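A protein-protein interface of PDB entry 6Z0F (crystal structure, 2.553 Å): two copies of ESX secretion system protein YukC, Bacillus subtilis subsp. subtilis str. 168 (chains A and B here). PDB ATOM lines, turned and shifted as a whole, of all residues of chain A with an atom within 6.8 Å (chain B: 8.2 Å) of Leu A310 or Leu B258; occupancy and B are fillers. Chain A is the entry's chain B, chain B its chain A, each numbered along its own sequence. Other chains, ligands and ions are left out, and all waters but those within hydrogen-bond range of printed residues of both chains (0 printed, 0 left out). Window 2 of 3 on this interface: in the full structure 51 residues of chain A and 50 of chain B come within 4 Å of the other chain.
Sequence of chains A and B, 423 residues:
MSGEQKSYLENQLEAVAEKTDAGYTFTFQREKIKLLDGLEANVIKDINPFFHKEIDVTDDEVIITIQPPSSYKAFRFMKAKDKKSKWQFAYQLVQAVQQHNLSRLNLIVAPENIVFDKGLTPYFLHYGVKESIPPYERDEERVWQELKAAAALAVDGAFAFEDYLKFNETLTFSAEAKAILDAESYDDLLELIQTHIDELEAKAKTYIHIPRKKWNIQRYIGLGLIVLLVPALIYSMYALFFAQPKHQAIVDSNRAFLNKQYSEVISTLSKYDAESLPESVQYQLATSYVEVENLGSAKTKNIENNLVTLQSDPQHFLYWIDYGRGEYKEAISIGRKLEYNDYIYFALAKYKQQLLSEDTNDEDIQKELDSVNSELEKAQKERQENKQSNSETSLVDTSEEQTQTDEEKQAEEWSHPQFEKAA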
ATOM      1  N   ASN A 254      33.040  -2.626   2.759  1.00  0.00           N
ATOM      2  CA  ASN A 254      32.769  -3.395   1.537  1.00  0.00           C
ATOM      3  C   ASN A 254      34.009  -4.200   1.126  1.00  0.00           C
ATOM      4  O   ASN A 254      33.859  -5.257   0.531  1.00  0.00           O
ATOM      5  CB  ASN A 254      32.279  -2.503   0.385  1.00  0.00           C
ATOM      6  CG  ASN A 254      30.893  -1.873   0.584  1.00  0.00           C
ATOM      7  OD1 ASN A 254      30.329  -1.261  -0.327  1.00  0.00           O
ATOM      8  ND2 ASN A 254      30.298  -1.987   1.772  1.00  0.00           N
ATOM      9  N   PHE A 257      34.124  -7.102   3.715  1.00  0.00           N
ATOM     10  CA  PHE A 257      33.066  -8.072   3.456  1.00  0.00           C
ATOM     11  C   PHE A 257      33.503  -9.045   2.373  1.00  0.00           C
ATOM     12  O   PHE A 257      33.283 -10.249   2.509  1.00  0.00           O
ATOM     13  CB  PHE A 257      31.761  -7.372   3.063  1.00  0.00           C
ATOM     14  CG  PHE A 257      30.631  -8.328   2.785  1.00  0.00           C
ATOM     15  CD1 PHE A 257      30.011  -9.006   3.815  1.00  0.00           C
ATOM     16  CD2 PHE A 257      30.198  -8.559   1.492  1.00  0.00           C
ATOM     17  CE1 PHE A 257      28.996  -9.906   3.555  1.00  0.00           C
ATOM     18  CE2 PHE A 257      29.169  -9.448   1.239  1.00  0.00           C
ATOM     19  CZ  PHE A 257      28.571 -10.113   2.272  1.00  0.00           C
ATOM     20  N   LEU A 258      34.151  -8.541   1.315  1.00  0.00           N
ATOM     21  CA  LEU A 258      34.630  -9.404   0.237  1.00  0.00           C
ATOM     22  C   LEU A 258      35.711 -10.380   0.719  1.00  0.00           C
ATOM     23  O   LEU A 258      35.832 -11.472   0.173  1.00  0.00           O
ATOM     24  CB  LEU A 258      35.165  -8.562  -0.926  1.00  0.00           C
ATOM     25  CG  LEU A 258      34.144  -7.703  -1.649  1.00  0.00           C
ATOM     26  CD1 LEU A 258      34.812  -6.867  -2.706  1.00  0.00           C
ATOM     27  CD2 LEU A 258      33.056  -8.549  -2.271  1.00  0.00           C
ATOM     28  N   GLU A 279      20.942   0.180   1.468  1.00  0.00           N
ATOM     29  CA  GLU A 279      20.427  -1.188   1.566  1.00  0.00           C
ATOM     30  C   GLU A 279      21.491  -2.264   1.272  1.00  0.00           C
ATOM     31  O   GLU A 279      21.508  -3.286   1.959  1.00  0.00           O
ATOM     32  CB  GLU A 279      19.217  -1.394   0.646  1.00  0.00           C
ATOM     33  CG  GLU A 279      17.884  -1.119   1.320  1.00  0.00           C
ATOM     34  CD  GLU A 279      16.680  -1.552   0.500  1.00  0.00           C
ATOM     35  OE1 GLU A 279      16.764  -2.613  -0.161  1.00  0.00           O
ATOM     36  OE2 GLU A 279      15.651  -0.834   0.516  1.00  0.00           O
ATOM     37  N   SER A 280      22.383  -2.043   0.288  1.00  0.00           N
ATOM     38  CA  SER A 280      23.434  -3.016  -0.019  1.00  0.00           C
ATOM     39  C   SER A 280      24.425  -3.136   1.137  1.00  0.00           C
ATOM     40  O   SER A 280      24.889  -4.233   1.437  1.00  0.00           O
ATOM     41  CB  SER A 280      24.165  -2.642  -1.301  1.00  0.00           C
ATOM     42  OG  SER A 280      24.758  -1.358  -1.215  1.00  0.00           O
ATOM     43  N   VAL A 281      24.725  -2.015   1.800  1.00  0.00           N
ATOM     44  CA  VAL A 281      25.622  -1.982   2.948  1.00  0.00           C
ATOM     45  C   VAL A 281      24.922  -2.636   4.161  1.00  0.00           C
ATOM     46  O   VAL A 281      25.562  -3.369   4.911  1.00  0.00           O
ATOM     47  CB  VAL A 281      26.084  -0.536   3.223  1.00  0.00           C
ATOM     48  CG1 VAL A 281      27.056  -0.480   4.390  1.00  0.00           C
ATOM     49  CG2 VAL A 281      26.723   0.061   1.972  1.00  0.00           C
ATOM     50  N   TYR A 283      22.795  -5.089   3.975  1.00  0.00           N
ATOM     51  CA  TYR A 283      22.870  -6.519   3.678  1.00  0.00           C
ATOM     52  C   TYR A 283      24.195  -7.084   4.197  1.00  0.00           C
ATOM     53  O   TYR A 283      24.204  -8.129   4.844  1.00  0.00           O
ATOM     54  CB  TYR A 283      22.708  -6.777   2.151  1.00  0.00           C
ATOM     55  CG  TYR A 283      23.383  -8.037   1.649  1.00  0.00           C
ATOM     56  CD1 TYR A 283      22.849  -9.288   1.912  1.00  0.00           C
ATOM     57  CD2 TYR A 283      24.585  -7.979   0.958  1.00  0.00           C
ATOM     58  CE1 TYR A 283      23.491 -10.449   1.501  1.00  0.00           C
ATOM     59  CE2 TYR A 283      25.239  -9.133   0.547  1.00  0.00           C
ATOM     60  CZ  TYR A 283      24.685 -10.369   0.814  1.00  0.00           C
ATOM     61  OH  TYR A 283      25.317 -11.516   0.396  1.00  0.00           O
ATOM     62  N   GLN A 284      25.306  -6.414   3.871  1.00  0.00           N
ATOM     63  CA  GLN A 284      26.635  -6.868   4.264  1.00  0.00           C
ATOM     64  C   GLN A 284      26.824  -6.802   5.760  1.00  0.00           C
ATOM     65  O   GLN A 284      27.514  -7.648   6.313  1.00  0.00           O
ATOM     66  CB  GLN A 284      27.719  -6.043   3.568  1.00  0.00           C
ATOM     67  CG  GLN A 284      27.587  -6.039   2.059  1.00  0.00           C
ATOM     68  CD  GLN A 284      28.554  -5.079   1.449  1.00  0.00           C
ATOM     69  OE1 GLN A 284      29.758  -5.138   1.700  1.00  0.00           O
ATOM     70  NE2 GLN A 284      28.046  -4.167   0.635  1.00  0.00           N
ATOM     71  N   GLU A 304      21.422 -16.995   5.307  1.00  0.00           N
ATOM     72  CA  GLU A 304      22.121 -16.293   4.243  1.00  0.00           C
ATOM     73  C   GLU A 304      21.546 -16.470   2.825  1.00  0.00           C
ATOM     74  O   GLU A 304      21.748 -15.564   2.012  1.00  0.00           O
ATOM     75  CB  GLU A 304      23.595 -16.678   4.244  1.00  0.00           C
ATOM     76  CG  GLU A 304      24.309 -16.145   5.469  1.00  0.00           C
ATOM     77  CD  GLU A 304      25.767 -16.533   5.589  1.00  0.00           C
ATOM     78  OE1 GLU A 304      26.237 -17.367   4.782  1.00  0.00           O
ATOM     79  OE2 GLU A 304      26.440 -16.005   6.502  1.00  0.00           O
ATOM     80  N   VAL A 308      18.360 -13.376   4.602  1.00  0.00           N
ATOM     81  CA  VAL A 308      19.188 -12.186   4.434  1.00  0.00           C
ATOM     82  C   VAL A 308      19.928 -12.261   3.100  1.00  0.00           C
ATOM     83  O   VAL A 308      21.103 -12.622   3.054  1.00  0.00           O
ATOM     84  CB  VAL A 308      20.152 -11.982   5.629  1.00  0.00           C
ATOM     85  CG1 VAL A 308      20.913 -10.666   5.508  1.00  0.00           C
ATOM     86  CG2 VAL A 308      19.392 -12.032   6.950  1.00  0.00           C
ATOM     87  N   THR A 309      19.216 -11.939   2.009  1.00  0.00           N
ATOM     88  CA  THR A 309      19.756 -11.919   0.648  1.00  0.00           C
ATOM     89  C   THR A 309      19.714 -10.499   0.060  1.00  0.00           C
ATOM     90  O   THR A 309      18.922  -9.670   0.501  1.00  0.00           O
ATOM     91  CB  THR A 309      18.975 -12.883  -0.250  1.00  0.00           C
ATOM     92  OG1 THR A 309      17.648 -12.389  -0.443  1.00  0.00           O
ATOM     93  CG2 THR A 309      18.929 -14.283   0.307  1.00  0.00           C
ATOM     94  N   LEU A 310      20.507 -10.242  -0.983  1.00  0.00           N
ATOM     95  CA  LEU A 310      20.546  -8.943  -1.654  1.00  0.00           C
ATOM     96  C   LEU A 310      19.185  -8.502  -2.215  1.00  0.00           C
ATOM     97  O   LEU A 310      18.998  -7.320  -2.485  1.00  0.00           O
ATOM     98  CB  LEU A 310      21.563  -8.988  -2.796  1.00  0.00           C
ATOM     99  CG  LEU A 310      23.012  -8.865  -2.389  1.00  0.00           C
ATOM    100  CD1 LEU A 310      23.889  -9.764  -3.232  1.00  0.00           C
ATOM    101  CD2 LEU A 310      23.460  -7.430  -2.457  1.00  0.00           C
ATOM    102  N   GLN A 311      18.249  -9.437  -2.401  1.00  0.00           N
ATOM    103  CA  GLN A 311      16.930  -9.123  -2.940  1.00  0.00           C
ATOM    104  C   GLN A 311      15.806  -9.233  -1.899  1.00  0.00           C
ATOM    105  O   GLN A 311      14.637  -9.142  -2.267  1.00  0.00           O
ATOM    106  CB  GLN A 311      16.629 -10.064  -4.110  1.00  0.00           C
ATOM    107  CG  GLN A 311      17.644  -9.939  -5.232  1.00  0.00           C
ATOM    108  CD  GLN A 311      17.305  -8.797  -6.159  1.00  0.00           C
ATOM    109  OE1 GLN A 311      16.134  -8.438  -6.355  1.00  0.00           O
ATOM    110  NE2 GLN A 311      18.322  -8.206  -6.770  1.00  0.00           N
ATOM    111  N   SER A 312      16.140  -9.422  -0.617  1.00  0.00           N
ATOM    112  CA  SER A 312      15.134  -9.563   0.429  1.00  0.00           C
ATOM    113  C   SER A 312      14.801  -8.227   1.104  1.00  0.00           C
ATOM    114  O   SER A 312      15.575  -7.275   1.018  1.00  0.00           O
ATOM    115  CB  SER A 312      15.599 -10.569   1.475  1.00  0.00           C
ATOM    116  OG  SER A 312      16.829 -10.167   2.050  1.00  0.00           O
ATOM    117  N   PHE A 317      17.513  -7.094   7.283  1.00  0.00           N
ATOM    118  CA  PHE A 317      18.823  -6.544   7.609  1.00  0.00           C
ATOM    119  C   PHE A 317      18.765  -5.802   8.931  1.00  0.00           C
ATOM    120  O   PHE A 317      19.660  -5.948   9.756  1.00  0.00           O
ATOM    121  CB  PHE A 317      19.336  -5.596   6.512  1.00  0.00           C
ATOM    122  CG  PHE A 317      19.222  -6.093   5.096  1.00  0.00           C
ATOM    123  CD1 PHE A 317      19.395  -7.431   4.797  1.00  0.00           C
ATOM    124  CD2 PHE A 317      19.017  -5.213   4.055  1.00  0.00           C
ATOM    125  CE1 PHE A 317      19.299  -7.883   3.490  1.00  0.00           C
ATOM    126  CE2 PHE A 317      18.923  -5.667   2.752  1.00  0.00           C
ATOM    127  CZ  PHE A 317      19.064  -6.997   2.477  1.00  0.00           C
ATOM    128  N   VAL B 251      29.018   2.849  -4.185  1.00  0.00           N
ATOM    129  CA  VAL B 251      27.947   2.098  -3.533  1.00  0.00           C
ATOM    130  C   VAL B 251      27.200   1.237  -4.580  1.00  0.00           C
ATOM    131  O   VAL B 251      27.003   0.040  -4.374  1.00  0.00           O
ATOM    132  CB  VAL B 251      26.995   3.084  -2.785  1.00  0.00           C
ATOM    133  CG1 VAL B 251      25.642   2.450  -2.476  1.00  0.00           C
ATOM    134  CG2 VAL B 251      27.646   3.616  -1.513  1.00  0.00           C
ATOM    135  N   ASP B 252      26.839   1.841  -5.714  1.00  0.00           N
ATOM    136  CA  ASP B 252      26.113   1.183  -6.795  1.00  0.00           C
ATOM    137  C   ASP B 252      26.927   0.093  -7.487  1.00  0.00           C
ATOM    138  O   ASP B 252      26.368  -0.949  -7.829  1.00  0.00           O
ATOM    139  CB  ASP B 252      25.649   2.205  -7.839  1.00  0.00           C
ATOM    140  CG  ASP B 252      24.580   3.156  -7.335  1.00  0.00           C
ATOM    141  OD1 ASP B 252      23.901   2.817  -6.338  1.00  0.00           O
ATOM    142  OD2 ASP B 252      24.430   4.251  -7.929  1.00  0.00           O
ATOM    143  N   SER B 253      28.227   0.326  -7.709  1.00  0.00           N
ATOM    144  CA  SER B 253      29.083  -0.665  -8.353  1.00  0.00           C
ATOM    145  C   SER B 253      29.383  -1.824  -7.409  1.00  0.00           C
ATOM    146  O   SER B 253      29.526  -2.950  -7.874  1.00  0.00           O
ATOM    147  CB  SER B 253      30.379  -0.033  -8.844  1.00  0.00           C
ATOM    148  OG  SER B 253      31.198   0.391  -7.769  1.00  0.00           O
ATOM    149  N   ASN B 254      29.471  -1.562  -6.091  1.00  0.00           N
ATOM    150  CA  ASN B 254      29.714  -2.605  -5.090  1.00  0.00           C
ATOM    151  C   ASN B 254      28.448  -3.443  -4.874  1.00  0.00           C
ATOM    152  O   ASN B 254      28.559  -4.624  -4.557  1.00  0.00           O
ATOM    153  CB  ASN B 254      30.233  -2.021  -3.768  1.00  0.00           C
ATOM    154  CG  ASN B 254      31.637  -1.430  -3.881  1.00  0.00           C
ATOM    155  OD1 ASN B 254      32.296  -1.504  -4.932  1.00  0.00           O
ATOM    156  ND2 ASN B 254      32.124  -0.810  -2.815  1.00  0.00           N
ATOM    157  N   ARG B 255      27.253  -2.857  -5.088  1.00  0.00           N
ATOM    158  CA  ARG B 255      25.988  -3.581  -4.996  1.00  0.00           C
ATOM    159  C   ARG B 255      25.831  -4.467  -6.233  1.00  0.00           C
ATOM    160  O   ARG B 255      25.454  -5.630  -6.113  1.00  0.00           O
ATOM    161  CB  ARG B 255      24.813  -2.599  -4.863  1.00  0.00           C
ATOM    162  CG  ARG B 255      23.422  -3.238  -5.031  1.00  0.00           C
ATOM    163  CD  ARG B 255      22.299  -2.209  -5.151  1.00  0.00           C
ATOM    164  NE  ARG B 255      22.640  -1.134  -6.088  1.00  0.00           N
ATOM    165  CZ  ARG B 255      22.241  -1.079  -7.353  1.00  0.00           C
ATOM    166  NH1 ARG B 255      22.651  -0.097  -8.139  1.00  0.00           N
ATOM    167  NH2 ARG B 255      21.421  -2.007  -7.841  1.00  0.00           N
ATOM    168  N   ALA B 256      26.137  -3.924  -7.420  1.00  0.00           N
ATOM    169  CA  ALA B 256      26.038  -4.683  -8.664  1.00  0.00           C
ATOM    170  C   ALA B 256      27.049  -5.826  -8.706  1.00  0.00           C
ATOM    171  O   ALA B 256      26.758  -6.865  -9.295  1.00  0.00           O
ATOM    172  CB  ALA B 256      26.242  -3.772  -9.856  1.00  0.00           C
ATOM    173  N   PHE B 257      28.218  -5.659  -8.071  1.00  0.00           N
ATOM    174  CA  PHE B 257      29.230  -6.710  -8.052  1.00  0.00           C
ATOM    175  C   PHE B 257      28.748  -7.889  -7.230  1.00  0.00           C
ATOM    176  O   PHE B 257      28.918  -9.032  -7.647  1.00  0.00           O
ATOM    177  CB  PHE B 257      30.568  -6.183  -7.513  1.00  0.00           C
ATOM    178  CG  PHE B 257      31.654  -7.232  -7.480  1.00  0.00           C
ATOM    179  CD1 PHE B 257      32.252  -7.671  -8.649  1.00  0.00           C
ATOM    180  CD2 PHE B 257      32.070  -7.789  -6.283  1.00  0.00           C
ATOM    181  CE1 PHE B 257      33.231  -8.653  -8.620  1.00  0.00           C
ATOM    182  CE2 PHE B 257      33.062  -8.759  -6.257  1.00  0.00           C
ATOM    183  CZ  PHE B 257      33.633  -9.186  -7.426  1.00  0.00           C
ATOM    184  N   LEU B 258      28.117  -7.620  -6.081  1.00  0.00           N
ATOM    185  CA  LEU B 258      27.597  -8.688  -5.229  1.00  0.00           C
ATOM    186  C   LEU B 258      26.471  -9.479  -5.919  1.00  0.00           C
ATOM    187  O   LEU B 258      26.295 -10.665  -5.642  1.00  0.00           O
ATOM    188  CB  LEU B 258      27.102  -8.122  -3.897  1.00  0.00           C
ATOM    189  CG  LEU B 258      28.165  -7.504  -3.004  1.00  0.00           C
ATOM    190  CD1 LEU B 258      27.542  -6.903  -1.772  1.00  0.00           C
ATOM    191  CD2 LEU B 258      29.224  -8.521  -2.619  1.00  0.00           C
ATOM    192  N   ASN B 259      25.732  -8.828  -6.829  1.00  0.00           N
ATOM    193  CA  ASN B 259      24.652  -9.453  -7.590  1.00  0.00           C
ATOM    194  C   ASN B 259      25.123 -10.066  -8.909  1.00  0.00           C
ATOM    195  O   ASN B 259      24.280 -10.369  -9.745  1.00  0.00           O
ATOM    196  CB  ASN B 259      23.575  -8.429  -7.890  1.00  0.00           C
ATOM    197  CG  ASN B 259      22.680  -8.162  -6.718  1.00  0.00           C
ATOM    198  OD1 ASN B 259      22.046  -9.073  -6.177  1.00  0.00           O
ATOM    199  ND2 ASN B 259      22.606  -6.907  -6.304  1.00  0.00           N
ATOM    200  N   LYS B 260      26.447 -10.234  -9.101  1.00  0.00           N
ATOM    201  CA  LYS B 260      27.067 -10.795 -10.299  1.00  0.00           C
ATOM    202  C   LYS B 260      26.609 -10.059 -11.566  1.00  0.00           C
ATOM    203  O   LYS B 260      26.404 -10.680 -12.607  1.00  0.00           O
ATOM    204  CB  LYS B 260      26.794 -12.302 -10.415  1.00  0.00           C
ATOM    205  CG  LYS B 260      27.349 -13.129  -9.264  1.00  0.00           C
ATOM    206  CD  LYS B 260      26.860 -14.580  -9.348  1.00  0.00           C
ATOM    207  CE  LYS B 260      26.060 -15.005  -8.133  1.00  0.00           C
ATOM    208  NZ  LYS B 260      25.426 -16.345  -8.310  1.00  0.00           N
ATOM    209  N   GLN B 261      26.424  -8.736 -11.467  1.00  0.00           N
ATOM    210  CA  GLN B 261      26.023  -7.879 -12.581  1.00  0.00           C
ATOM    211  C   GLN B 261      27.256  -7.137 -13.047  1.00  0.00           C
ATOM    212  O   GLN B 261      27.366  -5.929 -12.875  1.00  0.00           O
ATOM    213  CB  GLN B 261      24.913  -6.912 -12.141  1.00  0.00           C
ATOM    214  CG  GLN B 261      23.670  -7.620 -11.644  1.00  0.00           C
ATOM    215  CD  GLN B 261      22.800  -8.039 -12.792  1.00  0.00           C
ATOM    216  OE1 GLN B 261      22.386  -7.213 -13.618  1.00  0.00           O
ATOM    217  NE2 GLN B 261      22.511  -9.331 -12.868  1.00  0.00           N
ATOM    218  N   TYR B 262      28.194  -7.886 -13.615  1.00  0.00           N
ATOM    219  CA  TYR B 262      29.509  -7.412 -14.031  1.00  0.00           C
ATOM    220  C   TYR B 262      29.453  -6.294 -15.075  1.00  0.00           C
ATOM    221  O   TYR B 262      30.298  -5.400 -15.036  1.00  0.00           O
ATOM    222  CB  TYR B 262      30.359  -8.587 -14.534  1.00  0.00           C
ATOM    223  CG  TYR B 262      30.451  -9.698 -13.511  1.00  0.00           C
ATOM    224  CD1 TYR B 262      31.255  -9.571 -12.389  1.00  0.00           C
ATOM    225  CD2 TYR B 262      29.669 -10.839 -13.623  1.00  0.00           C
ATOM    226  CE1 TYR B 262      31.317 -10.573 -11.428  1.00  0.00           C
ATOM    227  CE2 TYR B 262      29.719 -11.845 -12.667  1.00  0.00           C
ATOM    228  CZ  TYR B 262      30.546 -11.709 -11.570  1.00  0.00           C
ATOM    229  OH  TYR B 262      30.600 -12.699 -10.619  1.00  0.00           O
ATOM    230  N   VAL B 265      28.614  -2.954 -13.205  1.00  0.00           N
ATOM    231  CA  VAL B 265      29.781  -2.426 -12.490  1.00  0.00           C
ATOM    232  C   VAL B 265      30.627  -1.577 -13.430  1.00  0.00           C
ATOM    233  O   VAL B 265      31.110  -0.514 -13.044  1.00  0.00           O
ATOM    234  CB  VAL B 265      30.626  -3.579 -11.911  1.00  0.00           C
ATOM    235  CG1 VAL B 265      31.867  -3.057 -11.193  1.00  0.00           C
ATOM    236  CG2 VAL B 265      29.799  -4.445 -10.988  1.00  0.00           C
ATOM    237  N   GLN B 284      37.055  -5.351  -8.101  1.00  0.00           N
ATOM    238  CA  GLN B 284      35.718  -5.645  -8.587  1.00  0.00           C
ATOM    239  C   GLN B 284      35.542  -5.214 -10.020  1.00  0.00           C
ATOM    240  O   GLN B 284      34.824  -5.879 -10.759  1.00  0.00           O
ATOM    241  CB  GLN B 284      34.665  -4.968  -7.709  1.00  0.00           C
ATOM    242  CG  GLN B 284      34.785  -5.328  -6.241  1.00  0.00           C
ATOM    243  CD  GLN B 284      33.845  -4.490  -5.421  1.00  0.00           C
ATOM    244  OE1 GLN B 284      32.641  -4.421  -5.683  1.00  0.00           O
ATOM    245  NE2 GLN B 284      34.375  -3.818  -4.414  1.00  0.00           N
ATOM    246  N   SER B 288      35.065  -7.836 -13.215  1.00  0.00           N
ATOM    247  CA  SER B 288      33.894  -7.585 -14.047  1.00  0.00           C
ATOM    248  C   SER B 288      34.307  -7.505 -15.519  1.00  0.00           C
ATOM    249  O   SER B 288      33.603  -8.043 -16.372  1.00  0.00           O
ATOM    250  CB  SER B 288      33.189  -6.310 -13.605  1.00  0.00           C
ATOM    251  OG  SER B 288      32.699  -6.451 -12.282  1.00  0.00           O
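Phe A257 touches Leu B258 (CE2 to CD2, 3.97 Å).
CD2 of Leu A258 touches CE2 of Phe B257, 3.99 Å away.
Leu A258 touches Leu B258.
Leu A258 touches Gln B284 (CD1 to NE2, 3.5 Å).
Arg B255 touches Ser A280.
Tyr A283 touches Leu B258 (CE2 to CD1, 3.96 Å).
Leu B258 touches Gln A284 (CD1 to NE2, 3.7 Å).
Leu B258 touches Leu A310.
CB of Leu A310 touches OD1 of Asn B259 (3.4 Å).
Gln A311 touches Asn B259.
ND2 of Asn B254 lies within hydrogen-bond range of OD1 of Asn A254 (3.1 Å).
OD1 of Asp B252 lies within salt-bridge range of NH1 of Arg B255, at 3.6 Å.
OD1 of Asn B254 lies close to OE1 of Gln B284, 3.0 Å away.
O of Arg B255 lies within hydrogen-bond range of ND2 of Asn B259.
The side-chain hydroxyl of Ser B288 sits at hydrogen-bond distance from the backbone carbonyl oxygen of Gln B284, at 2.7 Å.
The side-chain amide nitrogen (ND2) of Asn A254 is in hydrogen-bond range of the side-chain amide oxygen (OE1) of Gln A284, 3.2 Å away.
NE2 of Gln A284 sits at hydrogen-bond distance from O of Ser A280.
Leu A310 touches just these residues of chain B: Leu B258 and Asn B259.
Of chain A, only Phe A257 (3.97 Å), Leu A258 (3.8 Å), Tyr A283 (3.96 Å), Gln A284 (3.7 Å) and Leu A310 (3.5 Å) come within 4 Å of Leu B258.
Printed residues of chain B within 4 Å of Gln A311: Asn B259 (3.9 Å).
Printed residues of chain A within 4 Å of Arg B255: Ser A280 (3.6 Å).
Of the printed residues of chain B, Asn A254 touches Asn B254.
Printed residues of chain B within 4 Å of Leu A258: Phe B257, Leu B258 and Gln B284.
Printed residues of chain B within 4 Å of Ser A280: Arg B255 (3.6 Å).
Tyr B262 touches none of the printed residues of chain A.
The nearest residue of chain A that does not touch Leu B258 is Ser A280 (4.9 Å).
Asn B254 touches its own counterpart, Asn A254.
Phe A257 touches Leu B258, and with the chains exchanged Leu A258 touches Phe B257.
Leu B258 touches its own counterpart, Leu A258.
Leu A258 touches Gln B284, and with the chains exchanged Gln A284 touches Leu B258.
Hydrophobic or aromatic side chains of chain A within 4 Å of the printed part of chain B: Phe A257, Leu A258, Tyr A283 and Leu A310.
Hydrophobic or aromatic side chains of chain B within 4 Å of the printed part of chain A: Phe B257 and Leu B258.
Among the printed residues, 11 pairs touch across the chains.
Among the printed residues, no Asp or Glu carboxylate lies within 4 Å of a Lys or Arg side-chain nitrogen of the other chain.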
